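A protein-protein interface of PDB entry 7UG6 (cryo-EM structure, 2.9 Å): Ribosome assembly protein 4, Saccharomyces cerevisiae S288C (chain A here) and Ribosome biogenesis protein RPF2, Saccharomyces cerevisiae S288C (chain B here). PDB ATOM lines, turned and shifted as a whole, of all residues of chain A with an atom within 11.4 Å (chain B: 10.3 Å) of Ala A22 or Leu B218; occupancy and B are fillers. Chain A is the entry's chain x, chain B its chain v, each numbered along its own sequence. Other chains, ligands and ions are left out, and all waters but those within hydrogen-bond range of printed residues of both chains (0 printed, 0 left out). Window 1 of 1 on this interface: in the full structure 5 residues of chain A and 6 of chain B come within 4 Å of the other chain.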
ATOM      1  N   LEU A  17      35.353  -3.274 -37.176  1.00  0.00           N
ATOM      2  CA  LEU A  17      34.132  -3.650 -36.492  1.00  0.00           C
ATOM      3  C   LEU A  17      33.462  -2.420 -35.883  1.00  0.00           C
ATOM      4  O   LEU A  17      34.133  -1.441 -35.550  1.00  0.00           O
ATOM      5  CB  LEU A  17      34.419  -4.668 -35.394  1.00  0.00           C
ATOM      6  CG  LEU A  17      34.625  -6.122 -35.801  1.00  0.00           C
ATOM      7  CD1 LEU A  17      34.868  -6.967 -34.584  1.00  0.00           C
ATOM      8  CD2 LEU A  17      33.415  -6.622 -36.553  1.00  0.00           C
ATOM      9  N   PRO A  18      32.138  -2.440 -35.753  1.00  0.00           N
ATOM     10  CA  PRO A  18      31.458  -1.428 -34.937  1.00  0.00           C
ATOM     11  C   PRO A  18      31.998  -1.442 -33.518  1.00  0.00           C
ATOM     12  O   PRO A  18      31.796  -2.398 -32.769  1.00  0.00           O
ATOM     13  CB  PRO A  18      29.995  -1.869 -34.987  1.00  0.00           C
ATOM     14  CG  PRO A  18      29.888  -2.595 -36.273  1.00  0.00           C
ATOM     15  CD  PRO A  18      31.187  -3.288 -36.489  1.00  0.00           C
ATOM     16  N   ARG A  19      32.683  -0.367 -33.145  1.00  0.00           N
ATOM     17  CA  ARG A  19      33.603  -0.455 -32.023  1.00  0.00           C
ATOM     18  C   ARG A  19      33.573   0.836 -31.223  1.00  0.00           C
ATOM     19  O   ARG A  19      33.204   1.896 -31.735  1.00  0.00           O
ATOM     20  CB  ARG A  19      35.033  -0.763 -32.511  1.00  0.00           C
ATOM     21  CG  ARG A  19      36.051  -1.114 -31.422  1.00  0.00           C
ATOM     22  CD  ARG A  19      35.532  -2.160 -30.441  1.00  0.00           C
ATOM     23  NE  ARG A  19      35.461  -3.499 -31.017  1.00  0.00           N
ATOM     24  CZ  ARG A  19      36.326  -4.469 -30.737  1.00  0.00           C
ATOM     25  NH1 ARG A  19      37.326  -4.244 -29.895  1.00  0.00           N
ATOM     26  NH2 ARG A  19      36.195  -5.663 -31.295  1.00  0.00           N
ATOM     27  N   GLU A  20      33.964   0.712 -29.948  1.00  0.00           N
ATOM     28  CA  GLU A  20      34.168   1.817 -29.016  1.00  0.00           C
ATOM     29  C   GLU A  20      32.931   2.693 -28.879  1.00  0.00           C
ATOM     30  O   GLU A  20      33.047   3.899 -28.631  1.00  0.00           O
ATOM     31  CB  GLU A  20      35.377   2.670 -29.424  1.00  0.00           C
ATOM     32  CG  GLU A  20      36.739   2.004 -29.295  1.00  0.00           C
ATOM     33  CD  GLU A  20      37.171   1.815 -27.849  1.00  0.00           C
ATOM     34  OE1 GLU A  20      36.786   2.643 -26.996  1.00  0.00           O
ATOM     35  OE2 GLU A  20      37.911   0.849 -27.568  1.00  0.00           O
ATOM     36  N   VAL A  21      31.744   2.100 -29.021  1.00  0.00           N
ATOM     37  CA  VAL A  21      30.519   2.885 -29.070  1.00  0.00           C
ATOM     38  C   VAL A  21      30.212   3.417 -27.680  1.00  0.00           C
ATOM     39  O   VAL A  21      30.138   2.649 -26.711  1.00  0.00           O
ATOM     40  CB  VAL A  21      29.357   2.040 -29.604  1.00  0.00           C
ATOM     41  CG1 VAL A  21      28.077   2.854 -29.583  1.00  0.00           C
ATOM     42  CG2 VAL A  21      29.669   1.516 -30.991  1.00  0.00           C
ATOM     43  N   ALA A  22      30.041   4.736 -27.577  1.00  0.00           N
ATOM     44  CA  ALA A  22      29.808   5.358 -26.282  1.00  0.00           C
ATOM     45  C   ALA A  22      28.553   4.775 -25.655  1.00  0.00           C
ATOM     46  O   ALA A  22      27.564   4.494 -26.336  1.00  0.00           O
ATOM     47  CB  ALA A  22      29.684   6.875 -26.419  1.00  0.00           C
ATOM     48  N   ILE A  23      28.607   4.584 -24.335  1.00  0.00           N
ATOM     49  CA  ILE A  23      27.675   3.689 -23.663  1.00  0.00           C
ATOM     50  C   ILE A  23      26.236   4.194 -23.724  1.00  0.00           C
ATOM     51  O   ILE A  23      25.318   3.449 -23.355  1.00  0.00           O
ATOM     52  CB  ILE A  23      28.127   3.466 -22.207  1.00  0.00           C
ATOM     53  CG1 ILE A  23      27.664   2.100 -21.697  1.00  0.00           C
ATOM     54  CG2 ILE A  23      27.581   4.558 -21.318  1.00  0.00           C
ATOM     55  CD1 ILE A  23      28.369   0.934 -22.341  1.00  0.00           C
ATOM     56  N   ILE A  24      26.022   5.416 -24.222  1.00  0.00           N
ATOM     57  CA  ILE A  24      24.727   6.076 -24.426  1.00  0.00           C
ATOM     58  C   ILE A  24      23.785   5.768 -23.266  1.00  0.00           C
ATOM     59  O   ILE A  24      22.835   4.990 -23.435  1.00  0.00           O
ATOM     60  CB  ILE A  24      24.102   5.732 -25.795  1.00  0.00           C
ATOM     61  CG1 ILE A  24      24.168   4.243 -26.151  1.00  0.00           C
ATOM     62  CG2 ILE A  24      24.779   6.532 -26.883  1.00  0.00           C
ATOM     63  CD1 ILE A  24      23.433   3.872 -27.416  1.00  0.00           C
ATOM     64  N   PRO A  25      24.014   6.364 -22.093  1.00  0.00           N
ATOM     65  CA  PRO A  25      23.445   5.835 -20.843  1.00  0.00           C
ATOM     66  C   PRO A  25      21.934   5.673 -20.874  1.00  0.00           C
ATOM     67  O   PRO A  25      21.202   6.562 -21.310  1.00  0.00           O
ATOM     68  CB  PRO A  25      23.853   6.884 -19.802  1.00  0.00           C
ATOM     69  CG  PRO A  25      24.952   7.663 -20.434  1.00  0.00           C
ATOM     70  CD  PRO A  25      24.690   7.655 -21.892  1.00  0.00           C
ATOM     71  N   LYS A  26      21.473   4.521 -20.399  1.00  0.00           N
ATOM     72  CA  LYS A  26      20.050   4.330 -20.186  1.00  0.00           C
ATOM     73  C   LYS A  26      19.651   4.929 -18.839  1.00  0.00           C
ATOM     74  O   LYS A  26      20.460   5.048 -17.916  1.00  0.00           O
ATOM     75  CB  LYS A  26      19.686   2.846 -20.266  1.00  0.00           C
ATOM     76  CG  LYS A  26      18.190   2.571 -20.386  1.00  0.00           C
ATOM     77  CD  LYS A  26      17.615   3.207 -21.641  1.00  0.00           C
ATOM     78  CE  LYS A  26      18.131   2.520 -22.895  1.00  0.00           C
ATOM     79  NZ  LYS A  26      17.592   1.137 -23.027  1.00  0.00           N
ATOM     80  N   SER A  55      24.691  14.925 -15.167  1.00  0.00           N
ATOM     81  CA  SER A  55      25.877  15.434 -15.836  1.00  0.00           C
ATOM     82  C   SER A  55      26.690  16.308 -14.888  1.00  0.00           C
ATOM     83  O   SER A  55      26.249  16.671 -13.798  1.00  0.00           O
ATOM     84  CB  SER A  55      25.493  16.210 -17.092  1.00  0.00           C
ATOM     85  OG  SER A  55      26.645  16.723 -17.742  1.00  0.00           O
ATOM     86  N   TYR A 101      26.558   9.957 -18.379  1.00  0.00           N
ATOM     87  CA  TYR A 101      27.811   9.217 -18.355  1.00  0.00           C
ATOM     88  C   TYR A 101      28.861   9.990 -17.585  1.00  0.00           C
ATOM     89  O   TYR A 101      29.902   9.447 -17.213  1.00  0.00           O
ATOM     90  CB  TYR A 101      28.276   8.923 -19.781  1.00  0.00           C
ATOM     91  CG  TYR A 101      29.561   8.130 -19.901  1.00  0.00           C
ATOM     92  CD1 TYR A 101      29.589   6.770 -19.623  1.00  0.00           C
ATOM     93  CD2 TYR A 101      30.729   8.727 -20.354  1.00  0.00           C
ATOM     94  CE1 TYR A 101      30.752   6.036 -19.756  1.00  0.00           C
ATOM     95  CE2 TYR A 101      31.892   8.002 -20.489  1.00  0.00           C
ATOM     96  CZ  TYR A 101      31.898   6.657 -20.191  1.00  0.00           C
ATOM     97  OH  TYR A 101      33.059   5.934 -20.328  1.00  0.00           O
ATOM     98  N   SER A 102      28.568  11.267 -17.335  1.00  0.00           N
ATOM     99  CA  SER A 102      29.535  12.123 -16.665  1.00  0.00           C
ATOM    100  C   SER A 102      29.761  11.679 -15.231  1.00  0.00           C
ATOM    101  O   SER A 102      30.786  12.014 -14.631  1.00  0.00           O
ATOM    102  CB  SER A 102      29.075  13.580 -16.717  1.00  0.00           C
ATOM    103  OG  SER A 102      30.135  14.455 -16.372  1.00  0.00           O
ATOM    104  N   LEU A 104      28.654   8.137 -14.532  1.00  0.00           N
ATOM    105  CA  LEU A 104      28.076   6.802 -14.679  1.00  0.00           C
ATOM    106  C   LEU A 104      28.938   5.736 -14.018  1.00  0.00           C
ATOM    107  O   LEU A 104      28.530   5.105 -13.037  1.00  0.00           O
ATOM    108  CB  LEU A 104      27.904   6.479 -16.166  1.00  0.00           C
ATOM    109  CG  LEU A 104      27.185   5.216 -16.645  1.00  0.00           C
ATOM    110  CD1 LEU A 104      26.584   5.499 -17.984  1.00  0.00           C
ATOM    111  CD2 LEU A 104      28.106   4.018 -16.785  1.00  0.00           C
ATOM    112  N   ILE A 105      30.130   5.519 -14.562  1.00  0.00           N
ATOM    113  CA  ILE A 105      31.057   4.507 -14.076  1.00  0.00           C
ATOM    114  C   ILE A 105      32.381   5.225 -13.911  1.00  0.00           C
ATOM    115  O   ILE A 105      33.325   4.707 -13.305  1.00  0.00           O
ATOM    116  CB  ILE A 105      31.149   3.316 -15.049  1.00  0.00           C
ATOM    117  CG1 ILE A 105      31.729   2.084 -14.366  1.00  0.00           C
ATOM    118  CG2 ILE A 105      31.952   3.676 -16.277  1.00  0.00           C
ATOM    119  CD1 ILE A 105      31.545   0.830 -15.171  1.00  0.00           C
ATOM    120  N   LYS A 106      32.436   6.439 -14.447  1.00  0.00           N
ATOM    121  CA  LYS A 106      33.654   7.232 -14.362  1.00  0.00           C
ATOM    122  C   LYS A 106      34.059   7.572 -12.934  1.00  0.00           C
ATOM    123  O   LYS A 106      35.248   7.409 -12.613  1.00  0.00           O
ATOM    124  CB  LYS A 106      33.498   8.489 -15.228  1.00  0.00           C
ATOM    125  CG  LYS A 106      33.229   8.184 -16.709  1.00  0.00           C
ATOM    126  CD  LYS A 106      34.441   7.577 -17.446  1.00  0.00           C
ATOM    127  CE  LYS A 106      34.389   6.031 -17.480  1.00  0.00           C
ATOM    128  NZ  LYS A 106      35.463   5.373 -18.256  1.00  0.00           N
ATOM    129  N   VAL B 175      37.059  16.273 -38.083  1.00  0.00           N
ATOM    130  CA  VAL B 175      35.630  16.279 -37.786  1.00  0.00           C
ATOM    131  C   VAL B 175      34.975  17.529 -38.351  1.00  0.00           C
ATOM    132  O   VAL B 175      33.769  17.552 -38.611  1.00  0.00           O
ATOM    133  CB  VAL B 175      35.404  16.148 -36.271  1.00  0.00           C
ATOM    134  CG1 VAL B 175      33.948  15.896 -35.967  1.00  0.00           C
ATOM    135  CG2 VAL B 175      36.260  15.043 -35.714  1.00  0.00           C
ATOM    136  N   LYS B 207      23.812  19.354 -39.864  1.00  0.00           N
ATOM    137  CA  LYS B 207      23.783  20.329 -38.787  1.00  0.00           C
ATOM    138  C   LYS B 207      23.737  19.582 -37.471  1.00  0.00           C
ATOM    139  O   LYS B 207      22.917  18.681 -37.296  1.00  0.00           O
ATOM    140  CB  LYS B 207      22.584  21.257 -38.888  1.00  0.00           C
ATOM    141  CG  LYS B 207      22.669  22.215 -40.025  1.00  0.00           C
ATOM    142  CD  LYS B 207      21.546  23.217 -39.978  1.00  0.00           C
ATOM    143  CE  LYS B 207      21.734  24.251 -41.075  1.00  0.00           C
ATOM    144  NZ  LYS B 207      20.710  25.325 -41.045  1.00  0.00           N
ATOM    145  N   SER B 208      24.601  19.958 -36.545  1.00  0.00           N
ATOM    146  CA  SER B 208      24.685  19.259 -35.278  1.00  0.00           C
ATOM    147  C   SER B 208      24.232  20.163 -34.146  1.00  0.00           C
ATOM    148  O   SER B 208      24.790  21.241 -33.924  1.00  0.00           O
ATOM    149  CB  SER B 208      26.093  18.768 -35.005  1.00  0.00           C
ATOM    150  OG  SER B 208      26.569  18.029 -36.106  1.00  0.00           O
ATOM    151  N   TYR B 209      23.234  19.692 -33.413  1.00  0.00           N
ATOM    152  CA  TYR B 209      22.758  20.370 -32.229  1.00  0.00           C
ATOM    153  C   TYR B 209      23.102  19.518 -31.020  1.00  0.00           C
ATOM    154  O   TYR B 209      23.130  18.289 -31.093  1.00  0.00           O
ATOM    155  CB  TYR B 209      21.252  20.626 -32.289  1.00  0.00           C
ATOM    156  CG  TYR B 209      20.862  21.583 -33.378  1.00  0.00           C
ATOM    157  CD1 TYR B 209      20.028  21.192 -34.405  1.00  0.00           C
ATOM    158  CD2 TYR B 209      21.354  22.867 -33.394  1.00  0.00           C
ATOM    159  CE1 TYR B 209      19.673  22.065 -35.402  1.00  0.00           C
ATOM    160  CE2 TYR B 209      21.015  23.749 -34.394  1.00  0.00           C
ATOM    161  CZ  TYR B 209      20.175  23.344 -35.400  1.00  0.00           C
ATOM    162  OH  TYR B 209      19.829  24.222 -36.404  1.00  0.00           O
ATOM    163  N   LYS B 210      23.396  20.198 -29.916  1.00  0.00           N
ATOM    164  CA  LYS B 210      23.754  19.520 -28.684  1.00  0.00           C
ATOM    165  C   LYS B 210      22.598  18.636 -28.249  1.00  0.00           C
ATOM    166  O   LYS B 210      21.432  19.012 -28.371  1.00  0.00           O
ATOM    167  CB  LYS B 210      24.022  20.528 -27.574  1.00  0.00           C
ATOM    168  CG  LYS B 210      25.134  21.554 -27.798  1.00  0.00           C
ATOM    169  CD  LYS B 210      26.557  21.055 -27.788  1.00  0.00           C
ATOM    170  CE  LYS B 210      27.069  20.729 -29.174  1.00  0.00           C
ATOM    171  NZ  LYS B 210      28.492  20.359 -29.135  1.00  0.00           N
ATOM    172  N   SER B 211      22.917  17.464 -27.715  1.00  0.00           N
ATOM    173  CA  SER B 211      21.882  16.632 -27.114  1.00  0.00           C
ATOM    174  C   SER B 211      22.514  15.891 -25.952  1.00  0.00           C
ATOM    175  O   SER B 211      23.473  15.136 -26.139  1.00  0.00           O
ATOM    176  CB  SER B 211      21.286  15.669 -28.125  1.00  0.00           C
ATOM    177  OG  SER B 211      22.243  14.722 -28.550  1.00  0.00           O
ATOM    178  N   ASP B 212      21.970  16.098 -24.763  1.00  0.00           N
ATOM    179  CA  ASP B 212      22.571  15.589 -23.541  1.00  0.00           C
ATOM    180  C   ASP B 212      22.095  14.190 -23.184  1.00  0.00           C
ATOM    181  O   ASP B 212      21.990  13.854 -21.998  1.00  0.00           O
ATOM    182  CB  ASP B 212      22.343  16.591 -22.410  1.00  0.00           C
ATOM    183  CG  ASP B 212      20.888  16.807 -22.105  1.00  0.00           C
ATOM    184  OD1 ASP B 212      20.030  16.214 -22.798  1.00  0.00           O
ATOM    185  OD2 ASP B 212      20.606  17.590 -21.175  1.00  0.00           O
ATOM    186  N   GLN B 213      21.794  13.366 -24.188  1.00  0.00           N
ATOM    187  CA  GLN B 213      21.520  11.959 -23.927  1.00  0.00           C
ATOM    188  C   GLN B 213      22.801  11.198 -23.616  1.00  0.00           C
ATOM    189  O   GLN B 213      22.985  10.697 -22.501  1.00  0.00           O
ATOM    190  CB  GLN B 213      20.804  11.341 -25.120  1.00  0.00           C
ATOM    191  CG  GLN B 213      19.596  12.128 -25.546  1.00  0.00           C
ATOM    192  CD  GLN B 213      18.733  12.506 -24.365  1.00  0.00           C
ATOM    193  OE1 GLN B 213      18.698  13.665 -23.953  1.00  0.00           O
ATOM    194  NE2 GLN B 213      18.029  11.525 -23.807  1.00  0.00           N
ATOM    195  N   GLY B 214      23.701  11.107 -24.588  1.00  0.00           N
ATOM    196  CA  GLY B 214      24.967  10.439 -24.406  1.00  0.00           C
ATOM    197  C   GLY B 214      26.046  11.319 -23.823  1.00  0.00           C
ATOM    198  O   GLY B 214      27.136  10.823 -23.517  1.00  0.00           O
ATOM    199  N   GLY B 215      25.776  12.603 -23.654  1.00  0.00           N
ATOM    200  CA  GLY B 215      26.719  13.524 -23.073  1.00  0.00           C
ATOM    201  C   GLY B 215      27.206  14.553 -24.071  1.00  0.00           C
ATOM    202  O   GLY B 215      26.589  14.810 -25.107  1.00  0.00           O
ATOM    203  N   LYS B 216      28.345  15.151 -23.739  1.00  0.00           N
ATOM    204  CA  LYS B 216      28.988  16.139 -24.585  1.00  0.00           C
ATOM    205  C   LYS B 216      29.591  15.500 -25.827  1.00  0.00           C
ATOM    206  O   LYS B 216      29.846  16.196 -26.813  1.00  0.00           O
ATOM    207  CB  LYS B 216      30.093  16.843 -23.788  1.00  0.00           C
ATOM    208  CG  LYS B 216      30.714  18.095 -24.406  1.00  0.00           C
ATOM    209  CD  LYS B 216      29.751  18.909 -25.274  1.00  0.00           C
ATOM    210  CE  LYS B 216      28.727  19.632 -24.381  1.00  0.00           C
ATOM    211  NZ  LYS B 216      28.018  20.783 -24.996  1.00  0.00           N
ATOM    212  N   ARG B 217      29.792  14.181 -25.797  1.00  0.00           N
ATOM    213  CA  ARG B 217      30.598  13.506 -26.807  1.00  0.00           C
ATOM    214  C   ARG B 217      29.872  13.377 -28.138  1.00  0.00           C
ATOM    215  O   ARG B 217      30.475  13.564 -29.199  1.00  0.00           O
ATOM    216  CB  ARG B 217      31.011  12.131 -26.294  1.00  0.00           C
ATOM    217  CG  ARG B 217      31.655  12.181 -24.932  1.00  0.00           C
ATOM    218  CD  ARG B 217      33.025  12.838 -25.023  1.00  0.00           C
ATOM    219  NE  ARG B 217      34.008  12.017 -25.731  1.00  0.00           N
ATOM    220  CZ  ARG B 217      34.650  10.983 -25.189  1.00  0.00           C
ATOM    221  NH1 ARG B 217      34.415  10.636 -23.932  1.00  0.00           N
ATOM    222  NH2 ARG B 217      35.537  10.296 -25.899  1.00  0.00           N
ATOM    223  N   LEU B 218      28.600  13.026 -28.113  1.00  0.00           N
ATOM    224  CA  LEU B 218      27.880  12.723 -29.346  1.00  0.00           C
ATOM    225  C   LEU B 218      26.671  13.626 -29.520  1.00  0.00           C
ATOM    226  O   LEU B 218      25.744  13.593 -28.693  1.00  0.00           O
ATOM    227  CB  LEU B 218      27.527  11.235 -29.364  1.00  0.00           C
ATOM    228  CG  LEU B 218      26.653  10.501 -28.342  1.00  0.00           C
ATOM    229  CD1 LEU B 218      25.166  10.591 -28.575  1.00  0.00           C
ATOM    230  CD2 LEU B 218      27.090   9.054 -28.296  1.00  0.00           C
ATOM    231  N   PRO B 219      26.662  14.487 -30.526  1.00  0.00           N
ATOM    232  CA  PRO B 219      25.580  15.454 -30.676  1.00  0.00           C
ATOM    233  C   PRO B 219      24.406  14.851 -31.431  1.00  0.00           C
ATOM    234  O   PRO B 219      24.465  13.732 -31.936  1.00  0.00           O
ATOM    235  CB  PRO B 219      26.238  16.567 -31.494  1.00  0.00           C
ATOM    236  CG  PRO B 219      27.209  15.867 -32.327  1.00  0.00           C
ATOM    237  CD  PRO B 219      27.719  14.707 -31.525  1.00  0.00           C
ATOM    238  N   ARG B 220      23.326  15.618 -31.487  1.00  0.00           N
ATOM    239  CA  ARG B 220      22.191  15.223 -32.293  1.00  0.00           C
ATOM    240  C   ARG B 220      22.289  15.940 -33.617  1.00  0.00           C
ATOM    241  O   ARG B 220      22.495  17.153 -33.671  1.00  0.00           O
ATOM    242  CB  ARG B 220      20.869  15.569 -31.633  1.00  0.00           C
ATOM    243  CG  ARG B 220      19.729  14.778 -32.191  1.00  0.00           C
ATOM    244  CD  ARG B 220      18.900  15.511 -33.196  1.00  0.00           C
ATOM    245  NE  ARG B 220      17.723  14.715 -33.517  1.00  0.00           N
ATOM    246  CZ  ARG B 220      16.840  15.029 -34.453  1.00  0.00           C
ATOM    247  NH1 ARG B 220      17.007  16.123 -35.186  1.00  0.00           N
ATOM    248  NH2 ARG B 220      15.802  14.237 -34.665  1.00  0.00           N
ATOM    249  N   ILE B 221      22.130  15.187 -34.689  1.00  0.00           N
ATOM    250  CA  ILE B 221      22.445  15.685 -36.013  1.00  0.00           C
ATOM    251  C   ILE B 221      21.166  15.690 -36.831  1.00  0.00           C
ATOM    252  O   ILE B 221      20.373  14.745 -36.777  1.00  0.00           O
ATOM    253  CB  ILE B 221      23.569  14.845 -36.647  1.00  0.00           C
ATOM    254  CG1 ILE B 221      24.132  15.510 -37.870  1.00  0.00           C
ATOM    255  CG2 ILE B 221      23.099  13.510 -37.088  1.00  0.00           C
ATOM    256  CD1 ILE B 221      25.408  14.874 -38.247  1.00  0.00           C
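The side-chain amide oxygen of Gln B213 sits close to the side-chain carboxylate of Asp B212, 3.1 Å away.
CD2 of Leu B218 touches CB of Ala A22 (3.9 Å). CD2 of Leu B218 touches CG2 of Ile A24, at 3.7 Å. Gln B213 touches Pro A25 (O to CD, 3.5 Å). CD of Pro A25 touches CA of Gly B214, 3.8 Å away.
Of chain B, only Leu B218 (3.9 Å) comes within 4 Å of Ala A22. Of chain A, only Ala A22 (3.9 Å) and Ile A24 (3.7 Å) come within 4 Å of Leu B218. No residue of chain B comes within 4 Å of Ile A23. Of chain B, only Leu B218 (3.7 Å) comes within 4 Å of Ile A24. No residue of chain A comes within 4 Å of Ser B211. Gly B214 touches just one residue of chain A: Pro A25. Gly B215 touches none of the printed residues of chain A. No residue of chain A comes within 4 Å of Arg B217. No residue of chain A comes within 4 Å of Pro B219. Of the printed residues of chain A, Gln B213 touches Pro A25 (3.5 Å). Of the printed residues of chain B, Pro A25 touches Gln B213 (3.5 Å) and Gly B214 (3.8 Å). Lys A26 touches none of the printed residues of chain B. The nearest residue of chain B that does not touch Ala A22 is Arg B217 (5.4 Å). The nearest residue of chain A that does not touch Leu B218 is Ile A23 (6.2 Å). The nearest printed residue of chain B that does not touch Pro A25 is Gly B215 (5.4 Å).
Of the 16 printed residues of chain A, 3 touch a printed residue of chain B. Printed residues of chain A that touch a printed residue of chain B: Ala A22, Ile A24 and Pro A25. Hydrophobic or aromatic side chains of chain A that line the printed part of chain B: Ala A22, Ile A24 and Pro A25. Of the 16 printed residues of chain B, 3 touch a printed residue of chain A. Printed residues of chain B that touch a printed residue of chain A: Gln B213, Gly B214 and Leu B218. Hydrophobic or aromatic side chains of chain B that line the printed part of chain A: Leu B218. Among the printed residues, 4 pairs touch across the chains.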
